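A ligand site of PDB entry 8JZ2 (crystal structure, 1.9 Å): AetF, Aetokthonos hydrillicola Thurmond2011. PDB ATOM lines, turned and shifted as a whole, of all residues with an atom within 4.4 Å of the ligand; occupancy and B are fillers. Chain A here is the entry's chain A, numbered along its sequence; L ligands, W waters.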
ATOM      1  N   ILE A  18      25.922 -23.102 -14.464  1.00  0.00           N
ATOM      2  CA  ILE A  18      27.170 -22.333 -14.720  1.00  0.00           C
ATOM      3  C   ILE A  18      26.916 -21.450 -15.916  1.00  0.00           C
ATOM      4  O   ILE A  18      26.696 -21.975 -17.053  1.00  0.00           O
ATOM      5  CB  ILE A  18      28.368 -23.284 -14.914  1.00  0.00           C
ATOM      6  CG1 ILE A  18      28.649 -24.088 -13.649  1.00  0.00           C
ATOM      7  CG2 ILE A  18      29.612 -22.506 -15.362  1.00  0.00           C
ATOM      8  CD1 ILE A  18      29.518 -25.269 -13.915  1.00  0.00           C
ATOM      9  N   GLY A  19      26.903 -20.140 -15.682  1.00  0.00           N
ATOM     10  CA  GLY A  19      26.678 -19.152 -16.743  1.00  0.00           C
ATOM     11  C   GLY A  19      25.236 -18.719 -16.779  1.00  0.00           C
ATOM     12  O   GLY A  19      24.316 -19.580 -16.785  1.00  0.00           O
ATOM     13  N   PHE A  20      24.989 -17.410 -16.731  1.00  0.00           N
ATOM     14  CA  PHE A  20      23.610 -16.884 -16.678  1.00  0.00           C
ATOM     15  C   PHE A  20      23.576 -15.639 -17.541  1.00  0.00           C
ATOM     16  O   PHE A  20      24.208 -14.624 -17.216  1.00  0.00           O
ATOM     17  CB  PHE A  20      23.167 -16.613 -15.242  1.00  0.00           C
ATOM     18  CG  PHE A  20      21.692 -16.272 -15.174  1.00  0.00           C
ATOM     19  CD1 PHE A  20      21.253 -14.970 -15.389  1.00  0.00           C
ATOM     20  CD2 PHE A  20      20.751 -17.273 -15.015  1.00  0.00           C
ATOM     21  CE1 PHE A  20      19.906 -14.665 -15.355  1.00  0.00           C
ATOM     22  CE2 PHE A  20      19.403 -16.959 -14.977  1.00  0.00           C
ATOM     23  CZ  PHE A  20      18.989 -15.669 -15.116  1.00  0.00           C
ATOM     24  N   GLY A  21      22.981 -15.768 -18.707  1.00  0.00           N
ATOM     25  CA  GLY A  21      22.756 -14.602 -19.555  1.00  0.00           C
ATOM     26  C   GLY A  21      21.358 -14.647 -20.084  1.00  0.00           C
ATOM     27  O   GLY A  21      20.474 -13.889 -19.613  1.00  0.00           O
ATOM     28  N   PHE A  22      21.155 -15.467 -21.103  1.00  0.00           N
ATOM     29  CA  PHE A  22      19.853 -15.566 -21.800  1.00  0.00           C
ATOM     30  C   PHE A  22      19.364 -17.022 -21.769  1.00  0.00           C
ATOM     31  O   PHE A  22      18.179 -17.220 -21.461  1.00  0.00           O
ATOM     32  CB  PHE A  22      19.997 -15.032 -23.216  1.00  0.00           C
ATOM     33  CG  PHE A  22      18.783 -15.288 -24.070  1.00  0.00           C
ATOM     34  CD1 PHE A  22      17.574 -14.735 -23.748  1.00  0.00           C
ATOM     35  CD2 PHE A  22      18.832 -16.216 -25.098  1.00  0.00           C
ATOM     36  CE1 PHE A  22      16.448 -14.988 -24.528  1.00  0.00           C
ATOM     37  CE2 PHE A  22      17.705 -16.496 -25.867  1.00  0.00           C
ATOM     38  CZ  PHE A  22      16.527 -15.858 -25.587  1.00  0.00           C
ATOM     39  N   SER A  23      20.217 -17.996 -22.130  1.00  0.00           N
ATOM     40  CA  SER A  23      19.853 -19.432 -22.330  1.00  0.00           C
ATOM     41  C   SER A  23      19.302 -20.072 -21.046  1.00  0.00           C
ATOM     42  O   SER A  23      18.388 -20.926 -21.162  1.00  0.00           O
ATOM     43  CB  SER A  23      21.004 -20.236 -22.876  1.00  0.00           C
ATOM     44  OG  SER A  23      21.375 -19.764 -24.139  1.00  0.00           O
ATOM     45  N   ILE A  41      26.221 -20.024 -10.808  1.00  0.00           N
ATOM     46  CA  ILE A  41      27.559 -19.382 -10.777  1.00  0.00           C
ATOM     47  C   ILE A  41      27.728 -18.668 -12.103  1.00  0.00           C
ATOM     48  O   ILE A  41      27.619 -19.352 -13.149  1.00  0.00           O
ATOM     49  CB  ILE A  41      28.678 -20.409 -10.515  1.00  0.00           C
ATOM     50  CG1 ILE A  41      28.415 -21.248  -9.259  1.00  0.00           C
ATOM     51  CG2 ILE A  41      30.026 -19.687 -10.491  1.00  0.00           C
ATOM     52  CD1 ILE A  41      29.508 -22.248  -8.938  1.00  0.00           C
ATOM     53  N   SER A  42      27.993 -17.352 -12.106  1.00  0.00           N
ATOM     54  CA  SER A  42      28.171 -16.646 -13.390  1.00  0.00           C
ATOM     55  C   SER A  42      29.144 -15.477 -13.189  1.00  0.00           C
ATOM     56  O   SER A  42      29.038 -14.775 -12.151  1.00  0.00           O
ATOM     57  CB  SER A  42      26.842 -16.243 -13.985  1.00  0.00           C
ATOM     58  OG  SER A  42      26.997 -15.805 -15.335  1.00  0.00           O
ATOM     59  N   ALA A  43      30.023 -15.289 -14.178  1.00  0.00           N
ATOM     60  CA  ALA A  43      31.190 -14.386 -14.178  1.00  0.00           C
ATOM     61  C   ALA A  43      30.755 -12.946 -13.871  1.00  0.00           C
ATOM     62  O   ALA A  43      29.730 -12.541 -14.402  1.00  0.00           O
ATOM     63  CB  ALA A  43      31.856 -14.482 -15.524  1.00  0.00           C
ATOM     64  N   SER A  45      32.080 -10.415 -15.059  1.00  0.00           N
ATOM     65  CA  SER A  45      32.324  -9.682 -16.325  1.00  0.00           C
ATOM     66  C   SER A  45      31.078  -9.696 -17.230  1.00  0.00           C
ATOM     67  O   SER A  45      31.026  -8.858 -18.142  1.00  0.00           O
ATOM     68  CB  SER A  45      33.533 -10.225 -17.033  1.00  0.00           C
ATOM     69  OG  SER A  45      33.270 -11.538 -17.546  1.00  0.00           O
ATOM     70  N   GLY A  46      30.143 -10.627 -17.033  1.00  0.00           N
ATOM     71  CA  GLY A  46      28.979 -10.819 -17.927  1.00  0.00           C
ATOM     72  C   GLY A  46      29.388 -11.151 -19.351  1.00  0.00           C
ATOM     73  O   GLY A  46      30.378 -11.888 -19.546  1.00  0.00           O
ATOM     74  N   SER A  47      28.627 -10.640 -20.341  1.00  0.00           N
ATOM     75  CA  SER A  47      28.663 -11.071 -21.766  1.00  0.00           C
ATOM     76  C   SER A  47      29.011  -9.907 -22.692  1.00  0.00           C
ATOM     77  O   SER A  47      29.071  -8.759 -22.239  1.00  0.00           O
ATOM     78  CB  SER A  47      27.352 -11.637 -22.183  1.00  0.00           C
ATOM     79  OG  SER A  47      26.321 -10.645 -22.142  1.00  0.00           O
ATOM     80  N   VAL A  48      29.160 -10.228 -23.963  1.00  0.00           N
ATOM     81  CA  VAL A  48      29.267  -9.250 -25.077  1.00  0.00           C
ATOM     82  C   VAL A  48      28.182  -8.176 -24.929  1.00  0.00           C
ATOM     83  O   VAL A  48      28.507  -7.000 -25.153  1.00  0.00           O
ATOM     84  CB  VAL A  48      29.200  -9.976 -26.439  1.00  0.00           C
ATOM     85  CG1 VAL A  48      27.894 -10.722 -26.627  1.00  0.00           C
ATOM     86  CG2 VAL A  48      29.463  -9.022 -27.587  1.00  0.00           C
ATOM     87  N   TRP A  49      26.965  -8.539 -24.526  1.00  0.00           N
ATOM     88  CA  TRP A  49      25.845  -7.557 -24.394  1.00  0.00           C
ATOM     89  C   TRP A  49      26.234  -6.480 -23.374  1.00  0.00           C
ATOM     90  O   TRP A  49      25.870  -5.299 -23.583  1.00  0.00           O
ATOM     91  CB  TRP A  49      24.497  -8.219 -24.066  1.00  0.00           C
ATOM     92  CG  TRP A  49      24.071  -9.225 -25.076  1.00  0.00           C
ATOM     93  CD1 TRP A  49      24.160 -10.596 -24.976  1.00  0.00           C
ATOM     94  CD2 TRP A  49      23.523  -8.953 -26.372  1.00  0.00           C
ATOM     95  NE1 TRP A  49      23.716 -11.164 -26.130  1.00  0.00           N
ATOM     96  CE2 TRP A  49      23.321 -10.190 -27.002  1.00  0.00           C
ATOM     97  CE3 TRP A  49      23.161  -7.785 -27.039  1.00  0.00           C
ATOM     98  CZ2 TRP A  49      22.786 -10.287 -28.282  1.00  0.00           C
ATOM     99  CZ3 TRP A  49      22.651  -7.888 -28.304  1.00  0.00           C
ATOM    100  CH2 TRP A  49      22.452  -9.112 -28.914  1.00  0.00           C
ATOM    101  N   PHE A  60      21.686  -1.624 -32.813  1.00  0.00           N
ATOM    102  CA  PHE A  60      21.338  -2.538 -33.923  1.00  0.00           C
ATOM    103  C   PHE A  60      20.097  -3.335 -33.507  1.00  0.00           C
ATOM    104  O   PHE A  60      19.551  -3.038 -32.453  1.00  0.00           O
ATOM    105  CB  PHE A  60      22.529  -3.410 -34.318  1.00  0.00           C
ATOM    106  CG  PHE A  60      22.979  -4.409 -33.264  1.00  0.00           C
ATOM    107  CD1 PHE A  60      23.895  -4.029 -32.293  1.00  0.00           C
ATOM    108  CD2 PHE A  60      22.527  -5.721 -33.283  1.00  0.00           C
ATOM    109  CE1 PHE A  60      24.281  -4.913 -31.307  1.00  0.00           C
ATOM    110  CE2 PHE A  60      22.969  -6.634 -32.324  1.00  0.00           C
ATOM    111  CZ  PHE A  60      23.840  -6.235 -31.349  1.00  0.00           C
ATOM    112  N   LEU A  62      17.728  -7.315 -33.778  1.00  0.00           N
ATOM    113  CA  LEU A  62      17.836  -8.783 -33.996  1.00  0.00           C
ATOM    114  C   LEU A  62      17.481  -9.111 -35.456  1.00  0.00           C
ATOM    115  O   LEU A  62      16.753  -8.368 -36.106  1.00  0.00           O
ATOM    116  CB  LEU A  62      16.925  -9.513 -33.000  1.00  0.00           C
ATOM    117  CG  LEU A  62      17.098  -9.155 -31.519  1.00  0.00           C
ATOM    118  CD1 LEU A  62      16.285 -10.096 -30.634  1.00  0.00           C
ATOM    119  CD2 LEU A  62      18.540  -9.154 -31.084  1.00  0.00           C
ATOM    120  N   VAL A  63      17.991 -10.224 -35.948  1.00  0.00           N
ATOM    121  CA  VAL A  63      17.654 -10.783 -37.285  1.00  0.00           C
ATOM    122  C   VAL A  63      16.547 -11.817 -37.136  1.00  0.00           C
ATOM    123  O   VAL A  63      16.356 -12.596 -38.075  1.00  0.00           O
ATOM    124  CB  VAL A  63      18.924 -11.415 -37.888  1.00  0.00           C
ATOM    125  CG1 VAL A  63      20.025 -10.384 -38.029  1.00  0.00           C
ATOM    126  CG2 VAL A  63      19.410 -12.613 -37.099  1.00  0.00           C
ATOM    127  N   SER A  64      15.883 -11.850 -35.967  1.00  0.00           N
ATOM    128  CA  SER A  64      14.846 -12.840 -35.595  1.00  0.00           C
ATOM    129  C   SER A  64      13.633 -12.119 -35.014  1.00  0.00           C
ATOM    130  O   SER A  64      13.795 -11.058 -34.363  1.00  0.00           O
ATOM    131  CB  SER A  64      15.428 -13.852 -34.652  1.00  0.00           C
ATOM    132  OG  SER A  64      15.956 -13.233 -33.482  1.00  0.00           O
ATOM    133  N   SER A  69      12.124 -15.069 -30.385  1.00  0.00           N
ATOM    134  CA  SER A  69      13.354 -14.481 -29.778  1.00  0.00           C
ATOM    135  C   SER A  69      13.194 -14.172 -28.287  1.00  0.00           C
ATOM    136  O   SER A  69      14.230 -14.006 -27.609  1.00  0.00           O
ATOM    137  CB  SER A  69      13.743 -13.265 -30.549  1.00  0.00           C
ATOM    138  OG  SER A  69      14.014 -13.639 -31.891  1.00  0.00           O
ATOM    139  N   PHE A  90      16.433  -6.556 -26.407  1.00  0.00           N
ATOM    140  CA  PHE A  90      16.971  -7.914 -26.061  1.00  0.00           C
ATOM    141  C   PHE A  90      17.776  -7.816 -24.740  1.00  0.00           C
ATOM    142  O   PHE A  90      17.489  -8.541 -23.786  1.00  0.00           O
ATOM    143  CB  PHE A  90      17.758  -8.447 -27.258  1.00  0.00           C
ATOM    144  CG  PHE A  90      17.990  -9.928 -27.268  1.00  0.00           C
ATOM    145  CD1 PHE A  90      16.943 -10.821 -27.064  1.00  0.00           C
ATOM    146  CD2 PHE A  90      19.261 -10.436 -27.514  1.00  0.00           C
ATOM    147  CE1 PHE A  90      17.166 -12.181 -27.049  1.00  0.00           C
ATOM    148  CE2 PHE A  90      19.469 -11.820 -27.546  1.00  0.00           C
ATOM    149  CZ  PHE A  90      18.433 -12.674 -27.305  1.00  0.00           C
ATOM    150  N   ASP A 108      31.321 -15.496  -9.838  1.00  0.00           N
ATOM    151  CA  ASP A 108      32.640 -16.152  -9.900  1.00  0.00           C
ATOM    152  C   ASP A 108      32.720 -16.850 -11.241  1.00  0.00           C
ATOM    153  O   ASP A 108      31.717 -16.902 -11.972  1.00  0.00           O
ATOM    154  CB  ASP A 108      32.769 -17.176  -8.766  1.00  0.00           C
ATOM    155  CG  ASP A 108      34.166 -17.455  -8.221  1.00  0.00           C
ATOM    156  OD1 ASP A 108      35.164 -17.253  -8.940  1.00  0.00           O
ATOM    157  OD2 ASP A 108      34.213 -17.909  -7.066  1.00  0.00           O
ATOM    158  N   PHE A 109      33.881 -17.411 -11.522  1.00  0.00           N
ATOM    159  CA  PHE A 109      34.209 -18.008 -12.827  1.00  0.00           C
ATOM    160  C   PHE A 109      34.681 -19.437 -12.597  1.00  0.00           C
ATOM    161  O   PHE A 109      35.662 -19.682 -11.865  1.00  0.00           O
ATOM    162  CB  PHE A 109      35.273 -17.163 -13.509  1.00  0.00           C
ATOM    163  CG  PHE A 109      35.611 -17.622 -14.899  1.00  0.00           C
ATOM    164  CD1 PHE A 109      34.875 -17.179 -15.981  1.00  0.00           C
ATOM    165  CD2 PHE A 109      36.640 -18.519 -15.104  1.00  0.00           C
ATOM    166  CE1 PHE A 109      35.176 -17.633 -17.263  1.00  0.00           C
ATOM    167  CE2 PHE A 109      36.959 -18.941 -16.384  1.00  0.00           C
ATOM    168  CZ  PHE A 109      36.213 -18.513 -17.455  1.00  0.00           C
ATOM    169  N   VAL A 110      33.984 -20.370 -13.227  1.00  0.00           N
ATOM    170  CA  VAL A 110      34.325 -21.804 -13.140  1.00  0.00           C
ATOM    171  C   VAL A 110      35.498 -22.137 -14.072  1.00  0.00           C
ATOM    172  O   VAL A 110      35.407 -21.866 -15.264  1.00  0.00           O
ATOM    173  CB  VAL A 110      33.084 -22.639 -13.418  1.00  0.00           C
ATOM    174  CG1 VAL A 110      33.454 -24.116 -13.501  1.00  0.00           C
ATOM    175  CG2 VAL A 110      32.031 -22.390 -12.340  1.00  0.00           C
ATOM    176  N   ALA A 138      25.631 -23.213 -19.296  1.00  0.00           N
ATOM    177  CA  ALA A 138      24.908 -22.234 -20.129  1.00  0.00           C
ATOM    178  C   ALA A 138      25.828 -21.029 -20.375  1.00  0.00           C
ATOM    179  O   ALA A 138      25.421 -19.884 -20.072  1.00  0.00           O
ATOM    180  CB  ALA A 138      23.612 -21.881 -19.467  1.00  0.00           C
ATOM    181  N   THR A 139      27.033 -21.288 -20.861  1.00  0.00           N
ATOM    182  CA  THR A 139      28.134 -20.302 -20.854  1.00  0.00           C
ATOM    183  C   THR A 139      28.295 -19.614 -22.197  1.00  0.00           C
ATOM    184  O   THR A 139      29.220 -18.784 -22.294  1.00  0.00           O
ATOM    185  CB  THR A 139      29.450 -20.973 -20.446  1.00  0.00           C
ATOM    186  OG1 THR A 139      29.707 -22.035 -21.357  1.00  0.00           O
ATOM    187  CG2 THR A 139      29.462 -21.426 -19.003  1.00  0.00           C
ATOM    188  N   GLY A 140      27.516 -19.986 -23.201  1.00  0.00           N
ATOM    189  CA  GLY A 140      27.565 -19.388 -24.547  1.00  0.00           C
ATOM    190  C   GLY A 140      28.856 -19.742 -25.303  1.00  0.00           C
ATOM    191  O   GLY A 140      29.534 -20.718 -24.967  1.00  0.00           O
ATOM    192  N   ARG A 143      33.242 -15.841 -29.800  1.00  0.00           N
ATOM    193  CA  ARG A 143      33.112 -15.473 -31.233  1.00  0.00           C
ATOM    194  C   ARG A 143      34.195 -14.443 -31.568  1.00  0.00           C
ATOM    195  O   ARG A 143      34.234 -13.397 -30.892  1.00  0.00           O
ATOM    196  CB  ARG A 143      31.721 -14.899 -31.530  1.00  0.00           C
ATOM    197  CG  ARG A 143      30.594 -15.855 -31.191  1.00  0.00           C
ATOM    198  CD  ARG A 143      29.357 -15.603 -32.028  1.00  0.00           C
ATOM    199  NE  ARG A 143      28.442 -16.723 -31.920  1.00  0.00           N
ATOM    200  CZ  ARG A 143      27.538 -16.897 -30.942  1.00  0.00           C
ATOM    201  NH1 ARG A 143      26.745 -17.953 -30.941  1.00  0.00           N
ATOM    202  NH2 ARG A 143      27.428 -15.995 -29.981  1.00  0.00           N
ATOM    203  N   ASN A 146      33.245 -10.674 -32.250  1.00  0.00           N
ATOM    204  CA  ASN A 146      32.657  -9.777 -31.213  1.00  0.00           C
ATOM    205  C   ASN A 146      33.553  -8.518 -31.048  1.00  0.00           C
ATOM    206  O   ASN A 146      32.991  -7.411 -30.816  1.00  0.00           O
ATOM    207  CB  ASN A 146      32.355 -10.526 -29.916  1.00  0.00           C
ATOM    208  CG  ASN A 146      31.217 -11.530 -30.008  1.00  0.00           C
ATOM    209  OD1 ASN A 146      30.476 -11.599 -30.999  1.00  0.00           O
ATOM    210  ND2 ASN A 146      31.037 -12.335 -28.966  1.00  0.00           N
ATOM    211  N   ARG A 343      32.158 -21.922 -24.818  1.00  0.00           N
ATOM    212  CA  ARG A 343      33.018 -21.575 -23.680  1.00  0.00           C
ATOM    213  C   ARG A 343      32.894 -22.631 -22.589  1.00  0.00           C
ATOM    214  O   ARG A 343      32.325 -22.334 -21.537  1.00  0.00           O
ATOM    215  CB  ARG A 343      32.642 -20.214 -23.098  1.00  0.00           C
ATOM    216  CG  ARG A 343      33.135 -19.055 -23.929  1.00  0.00           C
ATOM    217  CD  ARG A 343      33.058 -17.768 -23.139  1.00  0.00           C
ATOM    218  NE  ARG A 343      31.649 -17.439 -22.968  1.00  0.00           N
ATOM    219  CZ  ARG A 343      30.955 -16.537 -23.675  1.00  0.00           C
ATOM    220  NH1 ARG A 343      31.529 -15.810 -24.615  1.00  0.00           N
ATOM    221  NH2 ARG A 343      29.674 -16.362 -23.398  1.00  0.00           N
ATOM    222  N   ARG A 381      22.141 -24.033 -32.451  1.00  0.00           N
ATOM    223  CA  ARG A 381      21.854 -22.743 -33.140  1.00  0.00           C
ATOM    224  C   ARG A 381      20.709 -22.988 -34.110  1.00  0.00           C
ATOM    225  O   ARG A 381      20.751 -23.949 -34.873  1.00  0.00           O
ATOM    226  CB  ARG A 381      23.070 -22.207 -33.903  1.00  0.00           C
ATOM    227  CG  ARG A 381      24.312 -22.109 -33.039  1.00  0.00           C
ATOM    228  CD  ARG A 381      25.231 -20.969 -33.434  1.00  0.00           C
ATOM    229  NE  ARG A 381      24.623 -19.720 -32.984  1.00  0.00           N
ATOM    230  CZ  ARG A 381      24.678 -18.563 -33.646  1.00  0.00           C
ATOM    231  NH1 ARG A 381      25.318 -18.485 -34.796  1.00  0.00           N
ATOM    232  NH2 ARG A 381      24.085 -17.498 -33.130  1.00  0.00           N
ATOM    233  N   GLY A 386      14.846 -16.990 -33.649  1.00  0.00           N
ATOM    234  CA  GLY A 386      15.710 -16.666 -32.507  1.00  0.00           C
ATOM    235  C   GLY A 386      16.141 -17.893 -31.755  1.00  0.00           C
ATOM    236  O   GLY A 386      15.503 -19.007 -31.884  1.00  0.00           O
ATOM    237  N   LEU A 387      17.139 -17.682 -30.913  1.00  0.00           N
ATOM    238  CA  LEU A 387      17.651 -18.705 -29.997  1.00  0.00           C
ATOM    239  C   LEU A 387      16.547 -19.156 -29.026  1.00  0.00           C
ATOM    240  O   LEU A 387      16.556 -20.380 -28.625  1.00  0.00           O
ATOM    241  CB  LEU A 387      18.880 -18.157 -29.280  1.00  0.00           C
ATOM    242  CG  LEU A 387      19.578 -19.178 -28.380  1.00  0.00           C
ATOM    243  CD1 LEU A 387      19.951 -20.456 -29.171  1.00  0.00           C
ATOM    244  CD2 LEU A 387      20.838 -18.548 -27.746  1.00  0.00           C
HETATM  245  P1  LIG L   1      25.650 -15.301 -22.839  1.00  0.00           P
HETATM  246  O1  LIG L   1      24.547 -14.332 -23.091  1.00  0.00           O
HETATM  247  O2  LIG L   1      26.982 -15.141 -23.442  1.00  0.00           O
HETATM  248  O3  LIG L   1      25.758 -15.553 -21.301  1.00  0.00           O
HETATM  249  C1  LIG L   1      26.685 -16.542 -20.749  1.00  0.00           C
HETATM  250  C2  LIG L   1      27.206 -16.054 -19.412  1.00  0.00           C
HETATM  251  O4  LIG L   1      28.063 -17.079 -18.834  1.00  0.00           O
HETATM  252  C3  LIG L   1      28.090 -14.795 -19.514  1.00  0.00           C
HETATM  253  O5  LIG L   1      27.657 -13.767 -18.635  1.00  0.00           O
HETATM  254  C4  LIG L   1      29.495 -15.303 -19.216  1.00  0.00           C
HETATM  255  O6  LIG L   1      30.321 -14.383 -18.570  1.00  0.00           O
HETATM  256  C5  LIG L   1      29.208 -16.472 -18.275  1.00  0.00           C
HETATM  257  N1  LIG L   1      30.260 -17.461 -18.249  1.00  0.00           N
HETATM  258  C6  LIG L   1      30.892 -18.028 -19.333  1.00  0.00           C
HETATM  259  N2  LIG L   1      31.795 -18.924 -18.988  1.00  0.00           N
HETATM  260  C7  LIG L   1      31.708 -18.961 -17.598  1.00  0.00           C
HETATM  261  C8  LIG L   1      32.393 -19.725 -16.637  1.00  0.00           C
HETATM  262  N3  LIG L   1      33.328 -20.613 -16.941  1.00  0.00           N
HETATM  263  N4  LIG L   1      32.098 -19.474 -15.343  1.00  0.00           N
HETATM  264  C9  LIG L   1      31.173 -18.570 -15.050  1.00  0.00           C
HETATM  265  N5  LIG L   1      30.457 -17.802 -15.875  1.00  0.00           N
HETATM  266  C10 LIG L   1      30.781 -18.065 -17.142  1.00  0.00           C
HETATM  267  N6  LIG L   1      20.139 -14.477 -31.047  1.00  0.00           N
HETATM  268  C11 LIG L   1      18.879 -14.253 -31.485  1.00  0.00           C
HETATM  269  O7  LIG L   1      17.952 -15.023 -31.155  1.00  0.00           O
HETATM  270  N7  LIG L   1      18.597 -13.283 -32.413  1.00  0.00           N
HETATM  271  C12 LIG L   1      19.550 -12.361 -32.809  1.00  0.00           C
HETATM  272  O8  LIG L   1      19.282 -11.501 -33.662  1.00  0.00           O
HETATM  273  C13 LIG L   1      20.844 -12.477 -32.244  1.00  0.00           C
HETATM  274  N8  LIG L   1      21.750 -11.569 -32.564  1.00  0.00           N
HETATM  275  C14 LIG L   1      22.968 -11.689 -31.948  1.00  0.00           C
HETATM  276  C15 LIG L   1      23.932 -10.703 -32.217  1.00  0.00           C
HETATM  277  C16 LIG L   1      25.181 -10.728 -31.639  1.00  0.00           C
HETATM  278  C17 LIG L   1      26.168  -9.618 -31.938  1.00  0.00           C
HETATM  279  C18 LIG L   1      25.523 -11.827 -30.785  1.00  0.00           C
HETATM  280  C19 LIG L   1      26.891 -11.934 -30.139  1.00  0.00           C
HETATM  281  C20 LIG L   1      24.603 -12.835 -30.562  1.00  0.00           C
HETATM  282  C21 LIG L   1      23.306 -12.783 -31.106  1.00  0.00           C
HETATM  283  N9  LIG L   1      22.327 -13.733 -30.819  1.00  0.00           N
HETATM  284  C22 LIG L   1      21.066 -13.597 -31.352  1.00  0.00           C
HETATM  285  C23 LIG L   1      22.697 -15.004 -30.143  1.00  0.00           C
HETATM  286  C24 LIG L   1      22.286 -15.252 -28.722  1.00  0.00           C
HETATM  287  O9  LIG L   1      20.970 -14.850 -28.439  1.00  0.00           O
HETATM  288  C25 LIG L   1      23.288 -14.554 -27.816  1.00  0.00           C
HETATM  289  O10 LIG L   1      24.598 -14.991 -28.144  1.00  0.00           O
HETATM  290  C26 LIG L   1      22.985 -14.831 -26.348  1.00  0.00           C
HETATM  291  O11 LIG L   1      23.857 -13.978 -25.625  1.00  0.00           O
HETATM  292  C27 LIG L   1      23.261 -16.267 -25.944  1.00  0.00           C
HETATM  293  O12 LIG L   1      22.959 -16.347 -24.525  1.00  0.00           O
HETATM  294  P2  LIG L   1      23.725 -17.344 -23.528  1.00  0.00           P
HETATM  295  O13 LIG L   1      22.982 -17.170 -22.263  1.00  0.00           O
HETATM  296  O14 LIG L   1      23.810 -18.654 -24.219  1.00  0.00           O
HETATM  297  O15 LIG L   1      25.193 -16.736 -23.412  1.00  0.00           O
HETATM  298  O   HOH W   1      24.352 -12.114 -21.357  1.00  0.00           O
HETATM  299  O   HOH W   2      25.999 -14.711 -32.680  1.00  0.00           O
HETATM  300  O   HOH W   3      16.199 -15.446 -28.976  1.00  0.00           O
HETATM  301  O   HOH W   4      24.960 -21.214 -23.428  1.00  0.00           O
HETATM  302  O   HOH W   5      33.750 -21.154 -19.700  1.00  0.00           O
HETATM  303  O   HOH W   6      23.695 -12.795 -35.015  1.00  0.00           O
HETATM  304  O   HOH W   7      22.842 -18.492 -19.855  1.00  0.00           O
HETATM  305  O   HOH W   8      24.807 -17.832 -28.839  1.00  0.00           O
HETATM  306  O   HOH W   9      25.391 -12.714 -18.936  1.00  0.00           O
HETATM  307  O   HOH W  10      19.095 -16.618 -33.767  1.00  0.00           O
HETATM  308  O   HOH W  11      21.484  -9.169 -34.348  1.00  0.00           O
HETATM  309  O   HOH W  12      27.689 -13.513 -15.962  1.00  0.00           O
HETATM  310  O   HOH W  13      26.662 -14.214 -26.271  1.00  0.00           O
HETATM  311  O   HOH W  14      25.402 -10.764 -35.141  1.00  0.00           O
HETATM  312  O   HOH W  15      24.734 -19.503 -26.602  1.00  0.00           O
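Merely in contact with the ligand: Ile 18 (3.9 Å), Gly 19 (3.3 Å), Phe 20 (3.7 Å), Gly 21 (3.6 Å), Ser 42 (3.6 Å), Ser 47 (3.7 Å), Val 48 (3.8 Å), Leu 62 (3.1 Å), Phe 90 (3.5 Å), Asp 108 (3.5 Å), Phe 109 (3.5 Å), Ala 138 (3.6 Å), Thr 139 (3.4 Å), Gly 140 (3.7 Å), Arg 143 (3.5 Å), Asn 146 (3.7 Å) and Gly 386 (3.1 Å).
Hydrophobic or aromatic side chains within 4 Å of the ligand: Ile 18, Phe 22, Ala 43, Val 48, Trp 49, Leu 62, Val 63, Phe 90, Phe 109, Val 110 and Leu 387.
Of the 32 residues printed, 27 come within 4 Å of the ligand.
N of Ser 23 lies within hydrogen-bond range of O13 of the ligand.
The side-chain hydroxyl (OG) of Ser 23 is in hydrogen-bond range of an oxygen (O14) of the ligand, 2.7 Å away.
An oxygen (O6) of the ligand sits at hydrogen-bond distance from the backbone carbonyl oxygen of Gly 46.
The backbone NH (N) of Phe 22 sits at hydrogen-bond distance from an oxygen (O13) of the ligand (2.8 Å).
N of Leu 387 sits at hydrogen-bond distance from O7 of the ligand, 2.8 Å away.
N7 of the ligand is in hydrogen-bond range of OG of Ser 64 (2.8 Å).
NE1 of Trp 49 lies within hydrogen-bond range of O11 of the ligand.
O8 of the ligand sits at hydrogen-bond distance from N of Val 63, 2.9 Å away.
N4 of the ligand sits at hydrogen-bond distance from N of Val 110, at 3.0 Å.
The backbone carbonyl oxygen of Val 110 is in hydrogen-bond range of a nitrogen (N3) of the ligand (3.0 Å).
NH2 of Arg 343 lies within salt-bridge range of O2 of the ligand (3.0 Å).
N5 of the ligand is in hydrogen-bond range of N of Ala 43 (3.1 Å).
OG of Ser 69 is in hydrogen-bond range of OG of Ser 64, 2.5 Å away.
N of Trp 49 sits close to OG of Ser 47, 3.2 Å away.
OG1 of Thr 139 lies within hydrogen-bond range of O of Arg 343, at 2.6 Å.
N of Arg 343 sits at hydrogen-bond distance from O of Gly 140 (2.9 Å).
The backbone NH (N) of Gly 19 lies within hydrogen-bond range of the backbone carbonyl oxygen (O) of Ile 41 (2.7 Å).
The backbone NH (N) of Asp 108 is in hydrogen-bond range of the backbone carbonyl oxygen (O) of Ser 42.
The side-chain hydroxyl (OG) of Ser 42 lies within hydrogen-bond range of the backbone NH (N) of Phe 20 (2.9 Å).
The backbone carbonyl oxygen (O) of Ile 18 sits at hydrogen-bond distance from the backbone NH (N) of Ala 138 (2.8 Å).
Water W9 bridges O5 of the ligand (2.5 Å) and O of Phe 20 (2.8 Å).
Water W12 lies within hydrogen-bond range of the side-chain hydroxyl of Ser 42 (2.5 Å), an oxygen (O5) of the ligand (2.7 Å) and the backbone carbonyl oxygen of Ala 43 (2.7 Å).
Water W7 lies within hydrogen-bond range of O13 of the ligand (2.8 Å), O of Ala 138 (2.9 Å) and N of Gly 21 (3.0 Å).
Water W3 lies within hydrogen-bond range of O of Ser 69 (2.8 Å), O7 of the ligand (2.8 Å) and N of Leu 387 (3.1 Å).
Water W5 bridges O of Arg 343 (2.6 Å) and N3 of the ligand (2.8 Å).
Water W4 lies within hydrogen-bond range of the backbone NH (N) of Gly 140 (2.8 Å), an oxygen (O14) of the ligand (2.9 Å) and the backbone NH (N) of Thr 139 (3.3 Å).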
